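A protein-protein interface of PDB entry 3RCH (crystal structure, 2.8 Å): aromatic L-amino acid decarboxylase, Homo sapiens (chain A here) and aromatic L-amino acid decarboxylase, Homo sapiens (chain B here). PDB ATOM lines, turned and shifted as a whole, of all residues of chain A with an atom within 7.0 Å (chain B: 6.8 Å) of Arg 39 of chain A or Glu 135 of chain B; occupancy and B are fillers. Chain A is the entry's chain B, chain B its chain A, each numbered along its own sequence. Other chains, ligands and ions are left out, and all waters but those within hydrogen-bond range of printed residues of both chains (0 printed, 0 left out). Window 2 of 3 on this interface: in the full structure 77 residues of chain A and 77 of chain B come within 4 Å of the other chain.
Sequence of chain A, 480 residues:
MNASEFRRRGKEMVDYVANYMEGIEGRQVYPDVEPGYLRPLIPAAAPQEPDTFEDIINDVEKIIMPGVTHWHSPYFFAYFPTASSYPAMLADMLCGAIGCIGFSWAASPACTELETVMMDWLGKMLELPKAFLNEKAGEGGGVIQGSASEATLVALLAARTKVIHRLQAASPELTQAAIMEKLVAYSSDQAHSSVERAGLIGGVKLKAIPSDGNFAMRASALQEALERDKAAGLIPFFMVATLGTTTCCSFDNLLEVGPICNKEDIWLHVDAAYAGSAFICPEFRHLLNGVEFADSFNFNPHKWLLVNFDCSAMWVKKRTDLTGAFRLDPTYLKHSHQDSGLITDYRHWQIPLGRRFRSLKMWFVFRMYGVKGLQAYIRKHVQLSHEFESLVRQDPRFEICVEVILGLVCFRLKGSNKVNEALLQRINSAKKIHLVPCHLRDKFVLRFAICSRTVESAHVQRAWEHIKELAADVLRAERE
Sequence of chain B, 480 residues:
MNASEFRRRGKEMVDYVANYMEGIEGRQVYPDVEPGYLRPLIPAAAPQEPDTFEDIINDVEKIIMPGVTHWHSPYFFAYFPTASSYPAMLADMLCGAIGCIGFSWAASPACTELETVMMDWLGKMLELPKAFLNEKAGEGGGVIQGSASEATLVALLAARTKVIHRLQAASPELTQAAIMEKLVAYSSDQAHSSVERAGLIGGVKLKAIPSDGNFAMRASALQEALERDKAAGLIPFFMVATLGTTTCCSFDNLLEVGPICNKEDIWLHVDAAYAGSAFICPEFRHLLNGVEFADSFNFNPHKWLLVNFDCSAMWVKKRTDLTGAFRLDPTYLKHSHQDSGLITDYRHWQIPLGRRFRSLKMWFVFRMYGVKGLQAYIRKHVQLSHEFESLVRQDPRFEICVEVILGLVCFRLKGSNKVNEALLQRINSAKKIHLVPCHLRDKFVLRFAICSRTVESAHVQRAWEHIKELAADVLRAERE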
ATOM      1  N   GLY A  36     -34.561  15.957 -13.514  1.00  0.00           N
ATOM      2  CA  GLY A  36     -33.471  15.219 -14.134  1.00  0.00           C
ATOM      3  C   GLY A  36     -33.293  15.623 -15.581  1.00  0.00           C
ATOM      4  O   GLY A  36     -32.244  15.381 -16.160  1.00  0.00           O
ATOM      5  N   TYR A  37     -34.299  16.266 -16.166  1.00  0.00           N
ATOM      6  CA  TYR A  37     -34.275  16.590 -17.597  1.00  0.00           C
ATOM      7  C   TYR A  37     -33.212  17.614 -17.979  1.00  0.00           C
ATOM      8  O   TYR A  37     -32.706  17.605 -19.098  1.00  0.00           O
ATOM      9  CB  TYR A  37     -35.647  17.101 -18.064  1.00  0.00           C
ATOM     10  CG  TYR A  37     -35.811  18.600 -17.964  1.00  0.00           C
ATOM     11  CD1 TYR A  37     -35.621  19.414 -19.073  1.00  0.00           C
ATOM     12  CD2 TYR A  37     -36.137  19.205 -16.755  1.00  0.00           C
ATOM     13  CE1 TYR A  37     -35.750  20.798 -18.980  1.00  0.00           C
ATOM     14  CE2 TYR A  37     -36.277  20.589 -16.653  1.00  0.00           C
ATOM     15  CZ  TYR A  37     -36.078  21.380 -17.767  1.00  0.00           C
ATOM     16  OH  TYR A  37     -36.222  22.747 -17.670  1.00  0.00           O
ATOM     17  N   LEU A  38     -32.888  18.496 -17.042  1.00  0.00           N
ATOM     18  CA  LEU A  38     -32.109  19.704 -17.329  1.00  0.00           C
ATOM     19  C   LEU A  38     -30.589  19.533 -17.476  1.00  0.00           C
ATOM     20  O   LEU A  38     -30.000  19.989 -18.462  1.00  0.00           O
ATOM     21  CB  LEU A  38     -32.386  20.757 -16.269  1.00  0.00           C
ATOM     22  CG  LEU A  38     -31.758  22.106 -16.565  1.00  0.00           C
ATOM     23  CD1 LEU A  38     -32.681  22.895 -17.472  1.00  0.00           C
ATOM     24  CD2 LEU A  38     -31.550  22.828 -15.287  1.00  0.00           C
ATOM     25  N   ARG A  39     -29.962  18.887 -16.500  1.00  0.00           N
ATOM     26  CA  ARG A  39     -28.514  18.681 -16.516  1.00  0.00           C
ATOM     27  C   ARG A  39     -27.874  18.349 -17.877  1.00  0.00           C
ATOM     28  O   ARG A  39     -26.885  18.972 -18.253  1.00  0.00           O
ATOM     29  CB  ARG A  39     -28.104  17.652 -15.455  1.00  0.00           C
ATOM     30  CG  ARG A  39     -26.631  17.672 -15.115  1.00  0.00           C
ATOM     31  CD  ARG A  39     -26.296  16.698 -14.006  1.00  0.00           C
ATOM     32  NE  ARG A  39     -26.322  17.305 -12.669  1.00  0.00           N
ATOM     33  CZ  ARG A  39     -25.358  18.077 -12.150  1.00  0.00           C
ATOM     34  NH1 ARG A  39     -24.278  18.396 -12.858  1.00  0.00           N
ATOM     35  NH2 ARG A  39     -25.482  18.551 -10.916  1.00  0.00           N
ATOM     36  N   PRO A  40     -28.423  17.376 -18.621  1.00  0.00           N
ATOM     37  CA  PRO A  40     -27.732  17.038 -19.854  1.00  0.00           C
ATOM     38  C   PRO A  40     -27.947  18.049 -20.982  1.00  0.00           C
ATOM     39  O   PRO A  40     -27.210  18.042 -21.968  1.00  0.00           O
ATOM     40  CB  PRO A  40     -28.334  15.680 -20.241  1.00  0.00           C
ATOM     41  CG  PRO A  40     -29.219  15.262 -19.086  1.00  0.00           C
ATOM     42  CD  PRO A  40     -29.608  16.525 -18.415  1.00  0.00           C
ATOM     43  N   LEU A  41     -28.940  18.916 -20.851  1.00  0.00           N
ATOM     44  CA  LEU A  41     -29.169  19.915 -21.882  1.00  0.00           C
ATOM     45  C   LEU A  41     -28.132  21.014 -21.805  1.00  0.00           C
ATOM     46  O   LEU A  41     -27.913  21.726 -22.764  1.00  0.00           O
ATOM     47  CB  LEU A  41     -30.589  20.470 -21.795  1.00  0.00           C
ATOM     48  CG  LEU A  41     -31.657  19.375 -21.994  1.00  0.00           C
ATOM     49  CD1 LEU A  41     -33.064  19.844 -21.615  1.00  0.00           C
ATOM     50  CD2 LEU A  41     -31.630  18.802 -23.422  1.00  0.00           C
ATOM     51  N   ILE A  42     -27.455  21.088 -20.669  1.00  0.00           N
ATOM     52  CA  ILE A  42     -26.581  22.198 -20.307  1.00  0.00           C
ATOM     53  C   ILE A  42     -25.164  21.703 -19.989  1.00  0.00           C
ATOM     54  O   ILE A  42     -25.015  20.721 -19.261  1.00  0.00           O
ATOM     55  CB  ILE A  42     -27.202  22.919 -19.090  1.00  0.00           C
ATOM     56  CG1 ILE A  42     -28.072  24.073 -19.566  1.00  0.00           C
ATOM     57  CG2 ILE A  42     -26.164  23.427 -18.104  1.00  0.00           C
ATOM     58  CD1 ILE A  42     -28.528  24.959 -18.421  1.00  0.00           C
ATOM     59  N   PRO A  43     -24.120  22.363 -20.532  1.00  0.00           N
ATOM     60  CA  PRO A  43     -22.746  21.881 -20.336  1.00  0.00           C
ATOM     61  C   PRO A  43     -22.367  21.653 -18.860  1.00  0.00           C
ATOM     62  O   PRO A  43     -23.017  22.177 -17.958  1.00  0.00           O
ATOM     63  CB  PRO A  43     -21.901  22.994 -20.949  1.00  0.00           C
ATOM     64  CG  PRO A  43     -22.776  23.569 -22.009  1.00  0.00           C
ATOM     65  CD  PRO A  43     -24.158  23.544 -21.415  1.00  0.00           C
ATOM     66  N   ALA A  44     -21.322  20.867 -18.628  1.00  0.00           N
ATOM     67  CA  ALA A  44     -20.958  20.395 -17.292  1.00  0.00           C
ATOM     68  C   ALA A  44     -20.225  21.431 -16.446  1.00  0.00           C
ATOM     69  O   ALA A  44     -20.144  21.281 -15.222  1.00  0.00           O
ATOM     70  CB  ALA A  44     -20.127  19.155 -17.407  1.00  0.00           C
ATOM     71  N   ALA A  45     -19.695  22.465 -17.104  1.00  0.00           N
ATOM     72  CA  ALA A  45     -18.885  23.514 -16.467  1.00  0.00           C
ATOM     73  C   ALA A  45     -19.182  24.867 -17.102  1.00  0.00           C
ATOM     74  O   ALA A  45     -19.681  24.926 -18.229  1.00  0.00           O
ATOM     75  CB  ALA A  45     -17.424  23.198 -16.606  1.00  0.00           C
ATOM     76  N   GLU B 113     -33.268  22.155 -10.518  1.00  0.00           N
ATOM     77  CA  GLU B 113     -32.202  21.593 -11.336  1.00  0.00           C
ATOM     78  C   GLU B 113     -31.117  22.577 -11.732  1.00  0.00           C
ATOM     79  O   GLU B 113     -29.939  22.259 -11.589  1.00  0.00           O
ATOM     80  CB  GLU B 113     -32.730  20.813 -12.532  1.00  0.00           C
ATOM     81  CG  GLU B 113     -32.683  19.310 -12.316  1.00  0.00           C
ATOM     82  CD  GLU B 113     -32.141  18.568 -13.527  1.00  0.00           C
ATOM     83  OE1 GLU B 113     -30.953  18.153 -13.501  1.00  0.00           O
ATOM     84  OE2 GLU B 113     -32.905  18.417 -14.510  1.00  0.00           O
ATOM     85  N   LEU B 114     -31.505  23.771 -12.186  1.00  0.00           N
ATOM     86  CA  LEU B 114     -30.542  24.787 -12.574  1.00  0.00           C
ATOM     87  C   LEU B 114     -29.726  25.227 -11.378  1.00  0.00           C
ATOM     88  O   LEU B 114     -28.553  25.553 -11.508  1.00  0.00           O
ATOM     89  CB  LEU B 114     -31.227  25.971 -13.228  1.00  0.00           C
ATOM     90  CG  LEU B 114     -30.334  27.047 -13.843  1.00  0.00           C
ATOM     91  CD1 LEU B 114     -29.463  26.486 -14.911  1.00  0.00           C
ATOM     92  CD2 LEU B 114     -31.172  28.172 -14.406  1.00  0.00           C
ATOM     93  N   THR B 116     -28.839  23.171  -8.707  1.00  0.00           N
ATOM     94  CA  THR B 116     -27.840  22.133  -8.482  1.00  0.00           C
ATOM     95  C   THR B 116     -26.658  22.296  -9.445  1.00  0.00           C
ATOM     96  O   THR B 116     -25.501  22.282  -9.016  1.00  0.00           O
ATOM     97  CB  THR B 116     -28.456  20.712  -8.666  1.00  0.00           C
ATOM     98  OG1 THR B 116     -29.772  20.675  -8.102  1.00  0.00           O
ATOM     99  CG2 THR B 116     -27.604  19.662  -8.001  1.00  0.00           C
ATOM    100  N   VAL B 117     -26.968  22.446 -10.736  1.00  0.00           N
ATOM    101  CA  VAL B 117     -25.975  22.562 -11.812  1.00  0.00           C
ATOM    102  C   VAL B 117     -25.158  23.846 -11.710  1.00  0.00           C
ATOM    103  O   VAL B 117     -23.974  23.848 -12.016  1.00  0.00           O
ATOM    104  CB  VAL B 117     -26.632  22.486 -13.224  1.00  0.00           C
ATOM    105  CG1 VAL B 117     -25.606  22.702 -14.295  1.00  0.00           C
ATOM    106  CG2 VAL B 117     -27.319  21.129 -13.453  1.00  0.00           C
ATOM    107  N   MET B 118     -25.790  24.937 -11.281  1.00  0.00           N
ATOM    108  CA  MET B 118     -25.086  26.207 -11.110  1.00  0.00           C
ATOM    109  C   MET B 118     -24.136  26.159  -9.921  1.00  0.00           C
ATOM    110  O   MET B 118     -23.010  26.652  -9.981  1.00  0.00           O
ATOM    111  CB  MET B 118     -26.066  27.375 -10.982  1.00  0.00           C
ATOM    112  CG  MET B 118     -26.649  27.881 -12.295  1.00  0.00           C
ATOM    113  SD  MET B 118     -25.459  28.028 -13.656  1.00  0.00           S
ATOM    114  CE  MET B 118     -25.656  26.444 -14.441  1.00  0.00           C
ATOM    115  N   ASP B 120     -22.779  23.484  -9.024  1.00  0.00           N
ATOM    116  CA  ASP B 120     -21.679  22.731  -9.576  1.00  0.00           C
ATOM    117  C   ASP B 120     -20.772  23.550 -10.478  1.00  0.00           C
ATOM    118  O   ASP B 120     -19.552  23.423 -10.385  1.00  0.00           O
ATOM    119  CB  ASP B 120     -22.148  21.451 -10.258  1.00  0.00           C
ATOM    120  CG  ASP B 120     -22.410  20.349  -9.268  1.00  0.00           C
ATOM    121  OD1 ASP B 120     -22.027  20.520  -8.098  1.00  0.00           O
ATOM    122  OD2 ASP B 120     -23.012  19.322  -9.636  1.00  0.00           O
ATOM    123  N   TRP B 121     -21.337  24.396 -11.339  1.00  0.00           N
ATOM    124  CA  TRP B 121     -20.497  25.343 -12.118  1.00  0.00           C
ATOM    125  C   TRP B 121     -19.560  26.127 -11.195  1.00  0.00           C
ATOM    126  O   TRP B 121     -18.336  26.081 -11.347  1.00  0.00           O
ATOM    127  CB  TRP B 121     -21.331  26.323 -12.968  1.00  0.00           C
ATOM    128  CG  TRP B 121     -21.829  25.735 -14.254  1.00  0.00           C
ATOM    129  CD1 TRP B 121     -21.967  24.416 -14.538  1.00  0.00           C
ATOM    130  CD2 TRP B 121     -22.292  26.445 -15.414  1.00  0.00           C
ATOM    131  NE1 TRP B 121     -22.473  24.257 -15.798  1.00  0.00           N
ATOM    132  CE2 TRP B 121     -22.686  25.485 -16.357  1.00  0.00           C
ATOM    133  CE3 TRP B 121     -22.421  27.805 -15.742  1.00  0.00           C
ATOM    134  CZ2 TRP B 121     -23.184  25.828 -17.612  1.00  0.00           C
ATOM    135  CZ3 TRP B 121     -22.923  28.150 -17.003  1.00  0.00           C
ATOM    136  CH2 TRP B 121     -23.294  27.166 -17.912  1.00  0.00           C
ATOM    137  N   LYS B 124     -16.859  24.129  -9.393  1.00  0.00           N
ATOM    138  CA  LYS B 124     -15.711  23.785 -10.222  1.00  0.00           C
ATOM    139  C   LYS B 124     -14.781  24.993 -10.386  1.00  0.00           C
ATOM    140  O   LYS B 124     -13.573  24.847 -10.583  1.00  0.00           O
ATOM    141  CB  LYS B 124     -16.174  23.262 -11.574  1.00  0.00           C
ATOM    142  CG  LYS B 124     -16.951  21.971 -11.499  1.00  0.00           C
ATOM    143  CD  LYS B 124     -17.236  21.426 -12.896  1.00  0.00           C
ATOM    144  CE  LYS B 124     -16.963  19.931 -12.969  1.00  0.00           C
ATOM    145  NZ  LYS B 124     -17.278  19.346 -14.310  1.00  0.00           N
ATOM    146  N   LYS B 130     -14.078  17.550  -4.577  1.00  0.00           N
ATOM    147  CA  LYS B 130     -15.256  16.886  -5.143  1.00  0.00           C
ATOM    148  C   LYS B 130     -16.345  16.515  -4.113  1.00  0.00           C
ATOM    149  O   LYS B 130     -17.517  16.369  -4.465  1.00  0.00           O
ATOM    150  CB  LYS B 130     -14.840  15.699  -6.007  1.00  0.00           C
ATOM    151  CG  LYS B 130     -14.349  16.146  -7.382  1.00  0.00           C
ATOM    152  CD  LYS B 130     -13.860  14.953  -8.220  1.00  0.00           C
ATOM    153  CE  LYS B 130     -13.201  15.419  -9.541  1.00  0.00           C
ATOM    154  NZ  LYS B 130     -11.948  14.647  -9.832  1.00  0.00           N
ATOM    155  N   LEU B 133     -19.420  18.596  -4.231  1.00  0.00           N
ATOM    156  CA  LEU B 133     -20.018  18.724  -5.548  1.00  0.00           C
ATOM    157  C   LEU B 133     -20.956  17.558  -5.808  1.00  0.00           C
ATOM    158  O   LEU B 133     -20.560  16.397  -5.651  1.00  0.00           O
ATOM    159  CB  LEU B 133     -18.903  18.713  -6.595  1.00  0.00           C
ATOM    160  CG  LEU B 133     -18.231  19.979  -7.128  1.00  0.00           C
ATOM    161  CD1 LEU B 133     -18.119  21.110  -6.111  1.00  0.00           C
ATOM    162  CD2 LEU B 133     -16.883  19.610  -7.706  1.00  0.00           C
ATOM    163  N   ASN B 134     -22.189  17.816  -6.215  1.00  0.00           N
ATOM    164  CA  ASN B 134     -23.001  16.665  -6.573  1.00  0.00           C
ATOM    165  C   ASN B 134     -23.351  16.592  -8.037  1.00  0.00           C
ATOM    166  O   ASN B 134     -24.497  16.746  -8.435  1.00  0.00           O
ATOM    167  CB  ASN B 134     -24.196  16.425  -5.629  1.00  0.00           C
ATOM    168  CG  ASN B 134     -25.411  17.307  -5.944  1.00  0.00           C
ATOM    169  OD1 ASN B 134     -25.361  18.551  -5.812  1.00  0.00           O
ATOM    170  ND2 ASN B 134     -26.527  16.655  -6.335  1.00  0.00           N
ATOM    171  N   GLU B 135     -22.326  16.366  -8.840  1.00  0.00           N
ATOM    172  CA  GLU B 135     -22.509  16.131 -10.261  1.00  0.00           C
ATOM    173  C   GLU B 135     -22.269  14.659 -10.508  1.00  0.00           C
ATOM    174  O   GLU B 135     -23.126  13.967 -11.066  1.00  0.00           O
ATOM    175  CB  GLU B 135     -21.556  16.989 -11.101  1.00  0.00           C
ATOM    176  CG  GLU B 135     -20.220  17.301 -10.423  1.00  0.00           C
ATOM    177  CD  GLU B 135     -19.079  17.434 -11.407  1.00  0.00           C
ATOM    178  OE1 GLU B 135     -19.351  17.693 -12.607  1.00  0.00           O
ATOM    179  OE2 GLU B 135     -17.916  17.272 -10.969  1.00  0.00           O
ATOM    180  N   LYS B 136     -21.105  14.177 -10.077  1.00  0.00           N
ATOM    181  CA  LYS B 136     -20.839  12.742 -10.086  1.00  0.00           C
ATOM    182  C   LYS B 136     -21.366  12.057  -8.799  1.00  0.00           C
ATOM    183  O   LYS B 136     -20.590  11.541  -7.985  1.00  0.00           O
ATOM    184  CB  LYS B 136     -19.353  12.447 -10.370  1.00  0.00           C
ATOM    185  CG  LYS B 136     -19.002  12.503 -11.869  1.00  0.00           C
ATOM    186  CD  LYS B 136     -17.533  12.861 -12.127  1.00  0.00           C
ATOM    187  CE  LYS B 136     -17.375  13.546 -13.493  1.00  0.00           C
ATOM    188  NZ  LYS B 136     -16.112  14.343 -13.572  1.00  0.00           N
ATOM    189  N   ALA B 137     -22.692  12.107  -8.622  1.00  0.00           N
ATOM    190  CA  ALA B 137     -23.410  11.253  -7.676  1.00  0.00           C
ATOM    191  C   ALA B 137     -22.972  11.377  -6.216  1.00  0.00           C
ATOM    192  O   ALA B 137     -23.292  10.504  -5.386  1.00  0.00           O
ATOM    193  CB  ALA B 137     -23.327   9.786  -8.136  1.00  0.00           C
ATOM    194  N   GLY B 138     -22.250  12.451  -5.897  1.00  0.00           N
ATOM    195  CA  GLY B 138     -21.645  12.578  -4.578  1.00  0.00           C
ATOM    196  C   GLY B 138     -22.667  12.602  -3.460  1.00  0.00           C
ATOM    197  O   GLY B 138     -23.843  12.877  -3.701  1.00  0.00           O
ATOM    198  N   GLY B 140     -22.580  14.851  -1.136  1.00  0.00           N
ATOM    199  CA  GLY B 140     -22.685  16.250  -0.704  1.00  0.00           C
ATOM    200  C   GLY B 140     -23.287  17.133  -1.783  1.00  0.00           C
ATOM    201  O   GLY B 140     -23.806  16.611  -2.777  1.00  0.00           O
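Printed residues of chain B within 4 Å of Gly 36 of chain A: Glu 113.
Of chain B, only Glu 113, Thr 116, Val 117, Asp 120, Asn 134 and Glu 135 come within 4 Å of Arg 39 of chain A.
Leu 41 of chain A touches none of the printed residues of chain B.
Of the printed residues of chain A, Leu 114 of chain B touches Leu 38 and Ile 42.
Of the printed residues of chain A, Asp 120 of chain B touches Arg 39.
Of the printed residues of chain A, Trp 121 of chain B touches Ile 42 (3.9 Å), Pro 43 (3.0 Å), Ala 44 (3.7 Å) and Ala 45 (3.6 Å).
Glu 135 of chain B touches just one residue of chain A: Arg 39.
Ala 137 of chain B touches none of the printed residues of chain A.
The side-chain carboxylate (OD2) of Asp 120 of chain B sits close to the backbone NH (N) of Glu 135 of chain B (3.1 Å).
The backbone NH of Asn 134 of chain B is in hydrogen-bond range of the side-chain carboxylate of Asp 120 of chain B, at 3.3 Å.
NZ of Lys 124 of chain B is in salt-bridge range of OE1 of Glu 135 of chain B.
Hydrophobic or aromatic side chains of chain A within 4 Å of the printed part of chain B: Leu 38 and Ile 42.
Of the 16 printed residues of chain B, 9 touch a printed residue of chain A.
Hydrophobic or aromatic side chains of chain B within 4 Å of the printed part of chain A: Leu 114, Val 117 and Trp 121.
Among the printed residues, 17 pairs touch across the chains.
Among the printed residues, Asp or Glu carboxylates within 4 Å of a Lys or Arg side-chain nitrogen of the other chain: Arg 39 of chain A with Asp 120 of chain B (2.9 Å).
Leu 38 of chain A touches Leu 114 of chain B (CD2 to N, 3.2 Å).
NH2 of Arg 39 of chain A touches CG2 of Thr 116 of chain B, 3.8 Å away.
Arg 39 of chain A touches Val 117 of chain B (CZ to CG2, 3.9 Å).
Arg 39 of chain A touches Glu 135 of chain B.
CD1 of Ile 42 of chain A touches CD1 of Leu 114 of chain B, at 3.9 Å.
Val 117 of chain B touches Ile 42 of chain A (CG1 to CG2, 3.9 Å).
Ile 42 of chain A touches Trp 121 of chain B.
Trp 121 of chain B touches Ala 44 of chain A.
O of Ala 44 of chain A touches NZ of Lys 124 of chain B, at 3.6 Å.
NE1 of Trp 121 of chain B touches N of Ala 45 of chain A, 3.6 Å away.
The backbone NH (N) of Tyr 37 of chain A lies within hydrogen-bond range of the side-chain carboxylate (OE2) of Glu 113 of chain B, 3.1 Å away.
OE2 of Glu 113 of chain B sits close to N of Gly 36 of chain A, 3.1 Å away.
The backbone carbonyl oxygen (O) of Asn 134 of chain B is in hydrogen-bond range of the guanidinium group (NH2) of Arg 39 of chain A (3.2 Å).
The side-chain carboxylate (OE2) of Glu 113 of chain B is in hydrogen-bond range of the backbone NH (N) of Leu 38 of chain A (2.5 Å).
The side-chain carboxylate of Glu 113 of chain B is in hydrogen-bond range of the backbone NH of Arg 39 of chain A, 3.2 Å away.
The backbone carbonyl oxygen (O) of Pro 43 of chain A lies within hydrogen-bond range of the indole nitrogen (NE1) of Trp 121 of chain B.
NH2 of Arg 39 of chain A is in salt-bridge range of OD2 of Asp 120 of chain B, 2.9 Å away.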
